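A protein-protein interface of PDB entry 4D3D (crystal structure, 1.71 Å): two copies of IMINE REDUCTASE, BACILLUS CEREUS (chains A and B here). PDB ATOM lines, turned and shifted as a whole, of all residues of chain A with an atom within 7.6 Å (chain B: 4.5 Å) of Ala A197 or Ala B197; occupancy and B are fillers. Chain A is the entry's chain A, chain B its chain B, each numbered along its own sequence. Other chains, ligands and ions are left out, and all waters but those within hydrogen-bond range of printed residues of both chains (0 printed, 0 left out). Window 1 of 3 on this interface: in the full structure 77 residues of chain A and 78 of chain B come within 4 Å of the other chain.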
ATOM      1  N   MET A 191       5.701   3.399  -4.435  1.00  0.00           N
ATOM      2  CA  MET A 191       6.834   4.209  -3.972  1.00  0.00           C
ATOM      3  C   MET A 191       6.386   5.590  -3.477  1.00  0.00           C
ATOM      4  O   MET A 191       7.009   6.119  -2.539  1.00  0.00           O
ATOM      5  CB  MET A 191       7.944   4.347  -5.026  1.00  0.00           C
ATOM      6  CG  MET A 191       8.619   3.033  -5.377  1.00  0.00           C
ATOM      7  SD  MET A 191       9.174   2.042  -3.941  1.00  0.00           S
ATOM      8  CE  MET A 191      10.408   3.118  -3.389  1.00  0.00           C
ATOM      9  N   ASP A 192       5.316   6.127  -4.013  1.00  0.00           N
ATOM     10  CA  ASP A 192       4.717   7.410  -3.509  1.00  0.00           C
ATOM     11  C   ASP A 192       4.374   7.231  -2.040  1.00  0.00           C
ATOM     12  O   ASP A 192       4.748   8.070  -1.177  1.00  0.00           O
ATOM     13  CB  ASP A 192       3.507   7.696  -4.351  1.00  0.00           C
ATOM     14  CG  ASP A 192       2.860   9.117  -4.202  1.00  0.00           C
ATOM     15  OD1 ASP A 192       3.441  10.040  -3.606  1.00  0.00           O
ATOM     16  OD2 ASP A 192       1.714   9.241  -4.805  1.00  0.00           O
ATOM     17  N   ILE A 193       3.690   6.139  -1.694  1.00  0.00           N
ATOM     18  CA  ILE A 193       3.344   5.815  -0.280  1.00  0.00           C
ATOM     19  C   ILE A 193       4.650   5.589   0.555  1.00  0.00           C
ATOM     20  O   ILE A 193       4.846   6.173   1.619  1.00  0.00           O
ATOM     21  CB  ILE A 193       2.423   4.592  -0.179  1.00  0.00           C
ATOM     22  CG1 ILE A 193       1.049   4.945  -0.775  1.00  0.00           C
ATOM     23  CG2 ILE A 193       2.234   4.206   1.247  1.00  0.00           C
ATOM     24  CD1 ILE A 193       0.070   3.742  -0.805  1.00  0.00           C
ATOM     25  N   PHE A 194       5.589   4.758   0.035  1.00  0.00           N
ATOM     26  CA  PHE A 194       6.760   4.439   0.732  1.00  0.00           C
ATOM     27  C   PHE A 194       7.521   5.679   1.204  1.00  0.00           C
ATOM     28  O   PHE A 194       7.818   5.800   2.431  1.00  0.00           O
ATOM     29  CB  PHE A 194       7.689   3.492  -0.038  1.00  0.00           C
ATOM     30  CG  PHE A 194       8.942   3.152   0.727  1.00  0.00           C
ATOM     31  CD1 PHE A 194       8.949   2.185   1.719  1.00  0.00           C
ATOM     32  CD2 PHE A 194      10.125   3.900   0.545  1.00  0.00           C
ATOM     33  CE1 PHE A 194      10.101   1.878   2.457  1.00  0.00           C
ATOM     34  CE2 PHE A 194      11.242   3.608   1.321  1.00  0.00           C
ATOM     35  CZ  PHE A 194      11.245   2.632   2.248  1.00  0.00           C
ATOM     36  N   TRP A 195       7.931   6.503   0.249  1.00  0.00           N
ATOM     37  CA  TRP A 195       8.777   7.612   0.572  1.00  0.00           C
ATOM     38  C   TRP A 195       8.059   8.650   1.445  1.00  0.00           C
ATOM     39  O   TRP A 195       8.657   9.229   2.349  1.00  0.00           O
ATOM     40  CB  TRP A 195       9.334   8.289  -0.656  1.00  0.00           C
ATOM     41  CG  TRP A 195      10.308   7.482  -1.407  1.00  0.00           C
ATOM     42  CD1 TRP A 195      10.192   7.092  -2.705  1.00  0.00           C
ATOM     43  CD2 TRP A 195      11.542   6.950  -0.932  1.00  0.00           C
ATOM     44  NE1 TRP A 195      11.295   6.385  -3.072  1.00  0.00           N
ATOM     45  CE2 TRP A 195      12.148   6.295  -2.022  1.00  0.00           C
ATOM     46  CE3 TRP A 195      12.219   7.021   0.243  1.00  0.00           C
ATOM     47  CZ2 TRP A 195      13.335   5.672  -1.904  1.00  0.00           C
ATOM     48  CZ3 TRP A 195      13.492   6.404   0.355  1.00  0.00           C
ATOM     49  CH2 TRP A 195      13.980   5.684  -0.699  1.00  0.00           C
ATOM     50  N   THR A 196       6.800   8.903   1.148  1.00  0.00           N
ATOM     51  CA  THR A 196       6.082   9.974   1.896  1.00  0.00           C
ATOM     52  C   THR A 196       5.833   9.530   3.313  1.00  0.00           C
ATOM     53  O   THR A 196       6.042  10.284   4.272  1.00  0.00           O
ATOM     54  CB  THR A 196       4.784  10.339   1.165  1.00  0.00           C
ATOM     55  OG1 THR A 196       5.042  10.615  -0.228  1.00  0.00           O
ATOM     56  CG2 THR A 196       4.146  11.605   1.799  1.00  0.00           C
ATOM     57  N   ALA A 197       5.400   8.257   3.492  1.00  0.00           N
ATOM     58  CA  ALA A 197       5.150   7.724   4.820  1.00  0.00           C
ATOM     59  C   ALA A 197       6.454   7.586   5.649  1.00  0.00           C
ATOM     60  O   ALA A 197       6.502   7.915   6.856  1.00  0.00           O
ATOM     61  CB  ALA A 197       4.413   6.436   4.732  1.00  0.00           C
ATOM     62  N   MET A 198       7.556   7.126   5.003  1.00  0.00           N
ATOM     63  CA  MET A 198       8.800   7.019   5.725  1.00  0.00           C
ATOM     64  C   MET A 198       9.370   8.377   6.113  1.00  0.00           C
ATOM     65  O   MET A 198       9.945   8.523   7.209  1.00  0.00           O
ATOM     66  CB  MET A 198       9.827   6.183   4.963  1.00  0.00           C
ATOM     67  CG  MET A 198       9.478   4.700   4.970  1.00  0.00           C
ATOM     68  SD  MET A 198       9.235   3.858   6.531  1.00  0.00           S
ATOM     69  CE  MET A 198      10.832   4.050   7.287  1.00  0.00           C
ATOM     70  N   LEU A 199       9.179   9.389   5.235  1.00  0.00           N
ATOM     71  CA  LEU A 199       9.655  10.712   5.650  1.00  0.00           C
ATOM     72  C   LEU A 199       8.784  11.228   6.807  1.00  0.00           C
ATOM     73  O   LEU A 199       9.288  11.938   7.688  1.00  0.00           O
ATOM     74  CB  LEU A 199       9.690  11.742   4.577  1.00  0.00           C
ATOM     75  CG  LEU A 199      11.079  12.092   3.984  1.00  0.00           C
ATOM     76  CD1 LEU A 199      11.906  10.925   3.649  1.00  0.00           C
ATOM     77  CD2 LEU A 199      10.928  13.109   2.826  1.00  0.00           C
ATOM     78  N   SER A 200       7.493  10.916   6.833  1.00  0.00           N
ATOM     79  CA  SER A 200       6.679  11.300   7.989  1.00  0.00           C
ATOM     80  C   SER A 200       7.084  10.688   9.285  1.00  0.00           C
ATOM     81  O   SER A 200       7.059  11.358  10.344  1.00  0.00           O
ATOM     82  CB  SER A 200       5.172  11.075   7.746  1.00  0.00           C
ATOM     83  OG  SER A 200       4.776   9.712   7.977  1.00  0.00           O
ATOM     84  N   TYR A 201       7.570   9.421   9.241  1.00  0.00           N
ATOM     85  CA  TYR A 201       8.213   8.791  10.396  1.00  0.00           C
ATOM     86  C   TYR A 201       9.428   9.544  10.867  1.00  0.00           C
ATOM     87  O   TYR A 201       9.588   9.796  12.084  1.00  0.00           O
ATOM     88  CB  TYR A 201       8.500   7.298  10.094  1.00  0.00           C
ATOM     89  CG  TYR A 201       9.448   6.703  11.078  1.00  0.00           C
ATOM     90  CD1 TYR A 201       9.029   6.378  12.349  1.00  0.00           C
ATOM     91  CD2 TYR A 201      10.814   6.565  10.767  1.00  0.00           C
ATOM     92  CE1 TYR A 201       9.976   5.892  13.273  1.00  0.00           C
ATOM     93  CE2 TYR A 201      11.741   6.035  11.678  1.00  0.00           C
ATOM     94  CZ  TYR A 201      11.290   5.714  12.917  1.00  0.00           C
ATOM     95  OH  TYR A 201      12.169   5.304  13.873  1.00  0.00           O
ATOM     96  N   LEU A 202      10.377   9.920   9.941  1.00  0.00           N
ATOM     97  CA  LEU A 202      11.581  10.618  10.325  1.00  0.00           C
ATOM     98  C   LEU A 202      11.232  11.983  10.899  1.00  0.00           C
ATOM     99  O   LEU A 202      11.819  12.387  11.892  1.00  0.00           O
ATOM    100  CB  LEU A 202      12.555  10.782   9.168  1.00  0.00           C
ATOM    101  CG  LEU A 202      13.106   9.440   8.632  1.00  0.00           C
ATOM    102  CD1 LEU A 202      13.906   9.727   7.404  1.00  0.00           C
ATOM    103  CD2 LEU A 202      14.025   8.739   9.635  1.00  0.00           C
ATOM    104  N   HIS A 203      10.209  12.608  10.321  1.00  0.00           N
ATOM    105  CA  HIS A 203       9.753  13.927  10.846  1.00  0.00           C
ATOM    106  C   HIS A 203       9.179  13.795  12.289  1.00  0.00           C
ATOM    107  O   HIS A 203       9.568  14.553  13.217  1.00  0.00           O
ATOM    108  CB  HIS A 203       8.684  14.469   9.886  1.00  0.00           C
ATOM    109  CG  HIS A 203       8.264  15.813  10.257  1.00  0.00           C
ATOM    110  ND1 HIS A 203       7.195  16.065  11.108  1.00  0.00           N
ATOM    111  CD2 HIS A 203       8.758  17.001   9.873  1.00  0.00           C
ATOM    112  CE1 HIS A 203       7.111  17.376  11.268  1.00  0.00           C
ATOM    113  NE2 HIS A 203       8.041  17.959  10.534  1.00  0.00           N
ATOM    114  N   MET A 225       0.856   2.451  14.564  1.00  0.00           N
ATOM    115  CA  MET A 225       0.110   3.371  13.746  1.00  0.00           C
ATOM    116  C   MET A 225       0.218   2.922  12.293  1.00  0.00           C
ATOM    117  O   MET A 225      -0.802   2.828  11.567  1.00  0.00           O
ATOM    118  CB  MET A 225       0.676   4.793  13.864  1.00  0.00           C
ATOM    119  CG  MET A 225       0.022   5.795  12.896  1.00  0.00           C
ATOM    120  SD  MET A 225      -1.781   5.813  13.009  1.00  0.00           S
ATOM    121  CE  MET A 225      -2.048   6.700  14.560  1.00  0.00           C
ATOM    122  N   MET A 226       1.435   2.579  11.828  1.00  0.00           N
ATOM    123  CA  MET A 226       1.603   2.091  10.464  1.00  0.00           C
ATOM    124  C   MET A 226       0.747   0.841  10.175  1.00  0.00           C
ATOM    125  O   MET A 226       0.137   0.757   9.124  1.00  0.00           O
ATOM    126  CB  MET A 226       3.082   1.769  10.166  1.00  0.00           C
ATOM    127  CG  MET A 226       3.976   2.993  10.198  1.00  0.00           C
ATOM    128  SD  MET A 226       3.732   4.082   8.817  1.00  0.00           S
ATOM    129  CE  MET A 226       5.292   5.006   8.795  1.00  0.00           C
ATOM    130  N   LEU A 229      -2.981   1.324   9.352  1.00  0.00           N
ATOM    131  CA  LEU A 229      -3.409   2.024   8.193  1.00  0.00           C
ATOM    132  C   LEU A 229      -4.205   1.168   7.208  1.00  0.00           C
ATOM    133  O   LEU A 229      -5.162   1.660   6.596  1.00  0.00           O
ATOM    134  CB  LEU A 229      -2.240   2.767   7.520  1.00  0.00           C
ATOM    135  CG  LEU A 229      -1.569   3.845   8.417  1.00  0.00           C
ATOM    136  CD1 LEU A 229      -0.519   4.601   7.682  1.00  0.00           C
ATOM    137  CD2 LEU A 229      -2.564   4.793   9.121  1.00  0.00           C
ATOM    138  N   VAL A 233      -7.720   2.017   4.934  1.00  0.00           N
ATOM    139  CA  VAL A 233      -7.772   1.845   3.506  1.00  0.00           C
ATOM    140  C   VAL A 233      -8.923   0.850   3.140  1.00  0.00           C
ATOM    141  O   VAL A 233      -9.665   1.162   2.279  1.00  0.00           O
ATOM    142  CB  VAL A 233      -6.431   1.336   2.940  1.00  0.00           C
ATOM    143  CG1 VAL A 233      -6.559   0.989   1.467  1.00  0.00           C
ATOM    144  CG2 VAL A 233      -5.372   2.439   3.084  1.00  0.00           C
ATOM    145  N   LEU A 275       6.991  19.695   5.630  1.00  0.00           N
ATOM    146  CA  LEU A 275       6.146  18.530   5.362  1.00  0.00           C
ATOM    147  C   LEU A 275       4.686  18.647   5.953  1.00  0.00           C
ATOM    148  O   LEU A 275       3.689  18.538   5.212  1.00  0.00           O
ATOM    149  CB  LEU A 275       6.834  17.202   5.801  1.00  0.00           C
ATOM    150  CG  LEU A 275       6.154  15.890   5.407  1.00  0.00           C
ATOM    151  CD1 LEU A 275       6.000  15.762   3.900  1.00  0.00           C
ATOM    152  CD2 LEU A 275       6.907  14.665   5.957  1.00  0.00           C
ATOM    153  N   VAL A 279       0.731  19.235   4.169  1.00  0.00           N
ATOM    154  CA  VAL A 279      -0.448  18.481   4.568  1.00  0.00           C
ATOM    155  C   VAL A 279      -1.562  19.516   4.944  1.00  0.00           C
ATOM    156  O   VAL A 279      -2.709  19.426   4.444  1.00  0.00           O
ATOM    157  CB  VAL A 279      -0.156  17.553   5.740  1.00  0.00           C
ATOM    158  CG1 VAL A 279      -1.393  16.912   6.303  1.00  0.00           C
ATOM    159  CG2 VAL A 279       0.879  16.447   5.304  1.00  0.00           C
ATOM    160  N   PHE A 296     -12.622  13.398   5.169  1.00  0.00           N
ATOM    161  CA  PHE A 296     -11.303  13.872   4.666  1.00  0.00           C
ATOM    162  C   PHE A 296     -10.900  13.124   3.400  1.00  0.00           C
ATOM    163  O   PHE A 296     -10.035  13.614   2.661  1.00  0.00           O
ATOM    164  CB  PHE A 296     -10.196  13.685   5.727  1.00  0.00           C
ATOM    165  CG  PHE A 296      -9.588  12.300   5.764  1.00  0.00           C
ATOM    166  CD1 PHE A 296     -10.132  11.277   6.506  1.00  0.00           C
ATOM    167  CD2 PHE A 296      -8.369  12.065   5.113  1.00  0.00           C
ATOM    168  CE1 PHE A 296      -9.554  10.026   6.565  1.00  0.00           C
ATOM    169  CE2 PHE A 296      -7.750  10.820   5.182  1.00  0.00           C
ATOM    170  CZ  PHE A 296      -8.354   9.792   5.889  1.00  0.00           C
ATOM    171  N   ILE B 193       2.267  10.973  11.462  1.00  0.00           N
ATOM    172  CA  ILE B 193       2.310   9.775  10.545  1.00  0.00           C
ATOM    173  C   ILE B 193       0.926   9.492   9.916  1.00  0.00           C
ATOM    174  O   ILE B 193       0.836   9.371   8.697  1.00  0.00           O
ATOM    175  CB  ILE B 193       2.832   8.569  11.286  1.00  0.00           C
ATOM    176  CG1 ILE B 193       4.291   8.757  11.681  1.00  0.00           C
ATOM    177  CG2 ILE B 193       2.714   7.356  10.407  1.00  0.00           C
ATOM    178  CD1 ILE B 193       4.869   7.640  12.558  1.00  0.00           C
ATOM    179  N   PHE B 194      -0.122   9.438  10.722  1.00  0.00           N
ATOM    180  CA  PHE B 194      -1.447   9.141  10.216  1.00  0.00           C
ATOM    181  C   PHE B 194      -1.836  10.000   9.058  1.00  0.00           C
ATOM    182  O   PHE B 194      -2.168   9.528   7.966  1.00  0.00           O
ATOM    183  CB  PHE B 194      -2.552   9.189  11.311  1.00  0.00           C
ATOM    184  CG  PHE B 194      -3.922   8.852  10.722  1.00  0.00           C
ATOM    185  CD1 PHE B 194      -4.299   7.514  10.631  1.00  0.00           C
ATOM    186  CD2 PHE B 194      -4.803   9.838  10.311  1.00  0.00           C
ATOM    187  CE1 PHE B 194      -5.546   7.183  10.101  1.00  0.00           C
ATOM    188  CE2 PHE B 194      -6.012   9.509   9.719  1.00  0.00           C
ATOM    189  CZ  PHE B 194      -6.364   8.176   9.627  1.00  0.00           C
ATOM    190  N   TRP B 195      -1.828  11.320   9.280  1.00  0.00           N
ATOM    191  CA  TRP B 195      -2.332  12.195   8.232  1.00  0.00           C
ATOM    192  C   TRP B 195      -1.424  12.273   6.977  1.00  0.00           C
ATOM    193  O   TRP B 195      -1.928  12.300   5.846  1.00  0.00           O
ATOM    194  CB  TRP B 195      -2.555  13.626   8.745  1.00  0.00           C
ATOM    195  CG  TRP B 195      -3.617  13.769   9.811  1.00  0.00           C
ATOM    196  CD1 TRP B 195      -3.450  14.241  11.076  1.00  0.00           C
ATOM    197  CD2 TRP B 195      -5.007  13.491   9.664  1.00  0.00           C
ATOM    198  NE1 TRP B 195      -4.667  14.310  11.715  1.00  0.00           N
ATOM    199  CE2 TRP B 195      -5.622  13.782  10.907  1.00  0.00           C
ATOM    200  CE3 TRP B 195      -5.787  12.991   8.629  1.00  0.00           C
ATOM    201  CZ2 TRP B 195      -6.995  13.600  11.128  1.00  0.00           C
ATOM    202  CZ3 TRP B 195      -7.204  12.824   8.849  1.00  0.00           C
ATOM    203  CH2 TRP B 195      -7.753  13.148  10.079  1.00  0.00           C
ATOM    204  N   THR B 196      -0.129  12.237   7.185  1.00  0.00           N
ATOM    205  CA  THR B 196       0.779  12.357   6.077  1.00  0.00           C
ATOM    206  C   THR B 196       0.721  11.070   5.252  1.00  0.00           C
ATOM    207  O   THR B 196       0.645  11.119   4.022  1.00  0.00           O
ATOM    208  CB  THR B 196       2.195  12.661   6.548  1.00  0.00           C
ATOM    209  OG1 THR B 196       2.234  13.801   7.455  1.00  0.00           O
ATOM    210  CG2 THR B 196       3.082  13.059   5.378  1.00  0.00           C
ATOM    211  N   ALA B 197       0.799   9.942   5.914  1.00  0.00           N
ATOM    212  CA  ALA B 197       0.728   8.642   5.207  1.00  0.00           C
ATOM    213  C   ALA B 197      -0.642   8.428   4.545  1.00  0.00           C
ATOM    214  O   ALA B 197      -0.719   7.988   3.374  1.00  0.00           O
ATOM    215  CB  ALA B 197       1.036   7.549   6.136  1.00  0.00           C
ATOM    216  N   MET B 198      -1.746   8.783   5.237  1.00  0.00           N
ATOM    217  CA  MET B 198      -3.046   8.621   4.572  1.00  0.00           C
ATOM    218  C   MET B 198      -3.252   9.565   3.395  1.00  0.00           C
ATOM    219  O   MET B 198      -3.826   9.176   2.328  1.00  0.00           O
ATOM    220  CB  MET B 198      -4.173   8.760   5.584  1.00  0.00           C
ATOM    221  CG  MET B 198      -4.298   7.565   6.474  1.00  0.00           C
ATOM    222  SD  MET B 198      -4.526   5.930   5.741  1.00  0.00           S
ATOM    223  CE  MET B 198      -6.095   6.173   4.902  1.00  0.00           C
ATOM    224  N   LEU B 199      -2.732  10.794   3.450  1.00  0.00           N
ATOM    225  CA  LEU B 199      -2.782  11.623   2.289  1.00  0.00           C
ATOM    226  C   LEU B 199      -1.943  11.025   1.133  1.00  0.00           C
ATOM    227  O   LEU B 199      -2.265  11.213  -0.042  1.00  0.00           O
ATOM    228  CB  LEU B 199      -2.288  13.081   2.482  1.00  0.00           C
ATOM    229  CG  LEU B 199      -3.288  14.000   3.187  1.00  0.00           C
ATOM    230  CD1 LEU B 199      -3.022  15.460   2.957  1.00  0.00           C
ATOM    231  CD2 LEU B 199      -4.695  13.631   3.088  1.00  0.00           C
ATOM    232  N   SER B 200      -0.815  10.406   1.461  1.00  0.00           N
ATOM    233  CA  SER B 200      -0.025   9.831   0.383  1.00  0.00           C
ATOM    234  C   SER B 200      -0.753   8.688  -0.311  1.00  0.00           C
ATOM    235  O   SER B 200      -0.611   8.527  -1.518  1.00  0.00           O
ATOM    236  CB  SER B 200       1.335   9.308   0.920  1.00  0.00           C
ATOM    237  OG  SER B 200       1.322   8.076   1.569  1.00  0.00           O
ATOM    238  N   TYR B 201      -1.549   7.949   0.436  1.00  0.00           N
ATOM    239  CA  TYR B 201      -2.468   6.910  -0.093  1.00  0.00           C
ATOM    240  C   TYR B 201      -3.475   7.536  -1.045  1.00  0.00           C
ATOM    241  O   TYR B 201      -3.652   7.081  -2.198  1.00  0.00           O
ATOM    242  CB  TYR B 201      -3.154   6.134   0.989  1.00  0.00           C
ATOM    243  CG  TYR B 201      -4.317   5.362   0.489  1.00  0.00           C
ATOM    244  CD1 TYR B 201      -4.143   4.240  -0.322  1.00  0.00           C
ATOM    245  CD2 TYR B 201      -5.633   5.866   0.657  1.00  0.00           C
ATOM    246  CE1 TYR B 201      -5.251   3.585  -0.891  1.00  0.00           C
ATOM    247  CE2 TYR B 201      -6.736   5.231   0.131  1.00  0.00           C
ATOM    248  CZ  TYR B 201      -6.572   4.106  -0.645  1.00  0.00           C
ATOM    249  OH  TYR B 201      -7.674   3.434  -1.211  1.00  0.00           O
ATOM    250  N   LEU B 229       5.865  -1.284   6.358  1.00  0.00           N
ATOM    251  CA  LEU B 229       6.663  -0.132   6.891  1.00  0.00           C
ATOM    252  C   LEU B 229       7.249  -0.362   8.280  1.00  0.00           C
ATOM    253  O   LEU B 229       8.371   0.014   8.519  1.00  0.00           O
ATOM    254  CB  LEU B 229       5.890   1.157   6.810  1.00  0.00           C
ATOM    255  CG  LEU B 229       5.442   1.604   5.389  1.00  0.00           C
ATOM    256  CD1 LEU B 229       4.695   2.887   5.417  1.00  0.00           C
ATOM    257  CD2 LEU B 229       6.566   1.638   4.371  1.00  0.00           C
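Ala A197 touches two residues of chain B.
Of the printed residues of chain A, Ala B197 touches Ala A197 (3.8 Å) and Leu A229 (3.7 Å).
Of the printed residues of chain B, Val A279 touches Thr B196 (3.7 Å) and Leu B199 (3.99 Å).
Of the printed residues of chain A, Leu B199 touches Val A279 (3.99 Å).
Printed residues of chain A within 4 Å of Tyr B201: Val A233.
His A203 touches none of the printed residues of chain B.
The nearest residue of chain A that does not touch Ala B197 is Ser A200 (4.5 Å).
Among the printed residues, pairs that only touch across the chains: Ile A193 with Ser B200, Phe A194 with Leu B229, Thr A196 with Ser B200, Ala A197 with Ala B197, Ala A197 with Leu B229, Ser A200 with Ile B193, Ser A200 with Thr B196, Met A225 with Ile B193, Met A225 with Phe B194, Met A226 with Ile B193, Met A226 with Leu B229, Leu A229 with Phe B194, Leu A229 with Ala B197, Val A233 with Tyr B201, Val A279 with Thr B196, Val A279 with Leu B199 and Phe A296 with Trp B195.
Of the 10 printed residues of chain B, 9 touch a printed residue of chain A.
Hydrophobic or aromatic side chains of chain B within 4 Å of the printed part of chain A: Ile B193, Phe B194, Trp B195, Ala B197, Leu B199, Tyr B201 and Leu B229.
Among the printed residues, 17 pairs touch across the chains.
Among the printed residues, no Asp or Glu carboxylate lies within 4 Å of a Lys or Arg side-chain nitrogen of the other chain.
Ile A193 touches Ser B200, and with the chains exchanged Ser A200 touches Ile B193.
Thr A196 touches Ser B200, and with the chains exchanged Ser A200 touches Thr B196.
Ala A197 touches its own counterpart, Ala B197.
Ala A197 touches Leu B229, and with the chains exchanged Leu A229 touches Ala B197.
Of the 17 pairs that touch across the chains among the printed residues, 9 have their exchanged pair printed and touching as well.
The backbone carbonyl oxygen (O) of Asp A192 sits at hydrogen-bond distance from the side-chain hydroxyl (OG1) of Thr A196.
The backbone carbonyl oxygen of Ala A197 lies within hydrogen-bond range of the side-chain hydroxyl of Ser A200, at 2.7 Å.
The backbone carbonyl oxygen (O) of Ala B197 sits at hydrogen-bond distance from the side-chain hydroxyl (OG) of Ser B200, at 2.7 Å.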
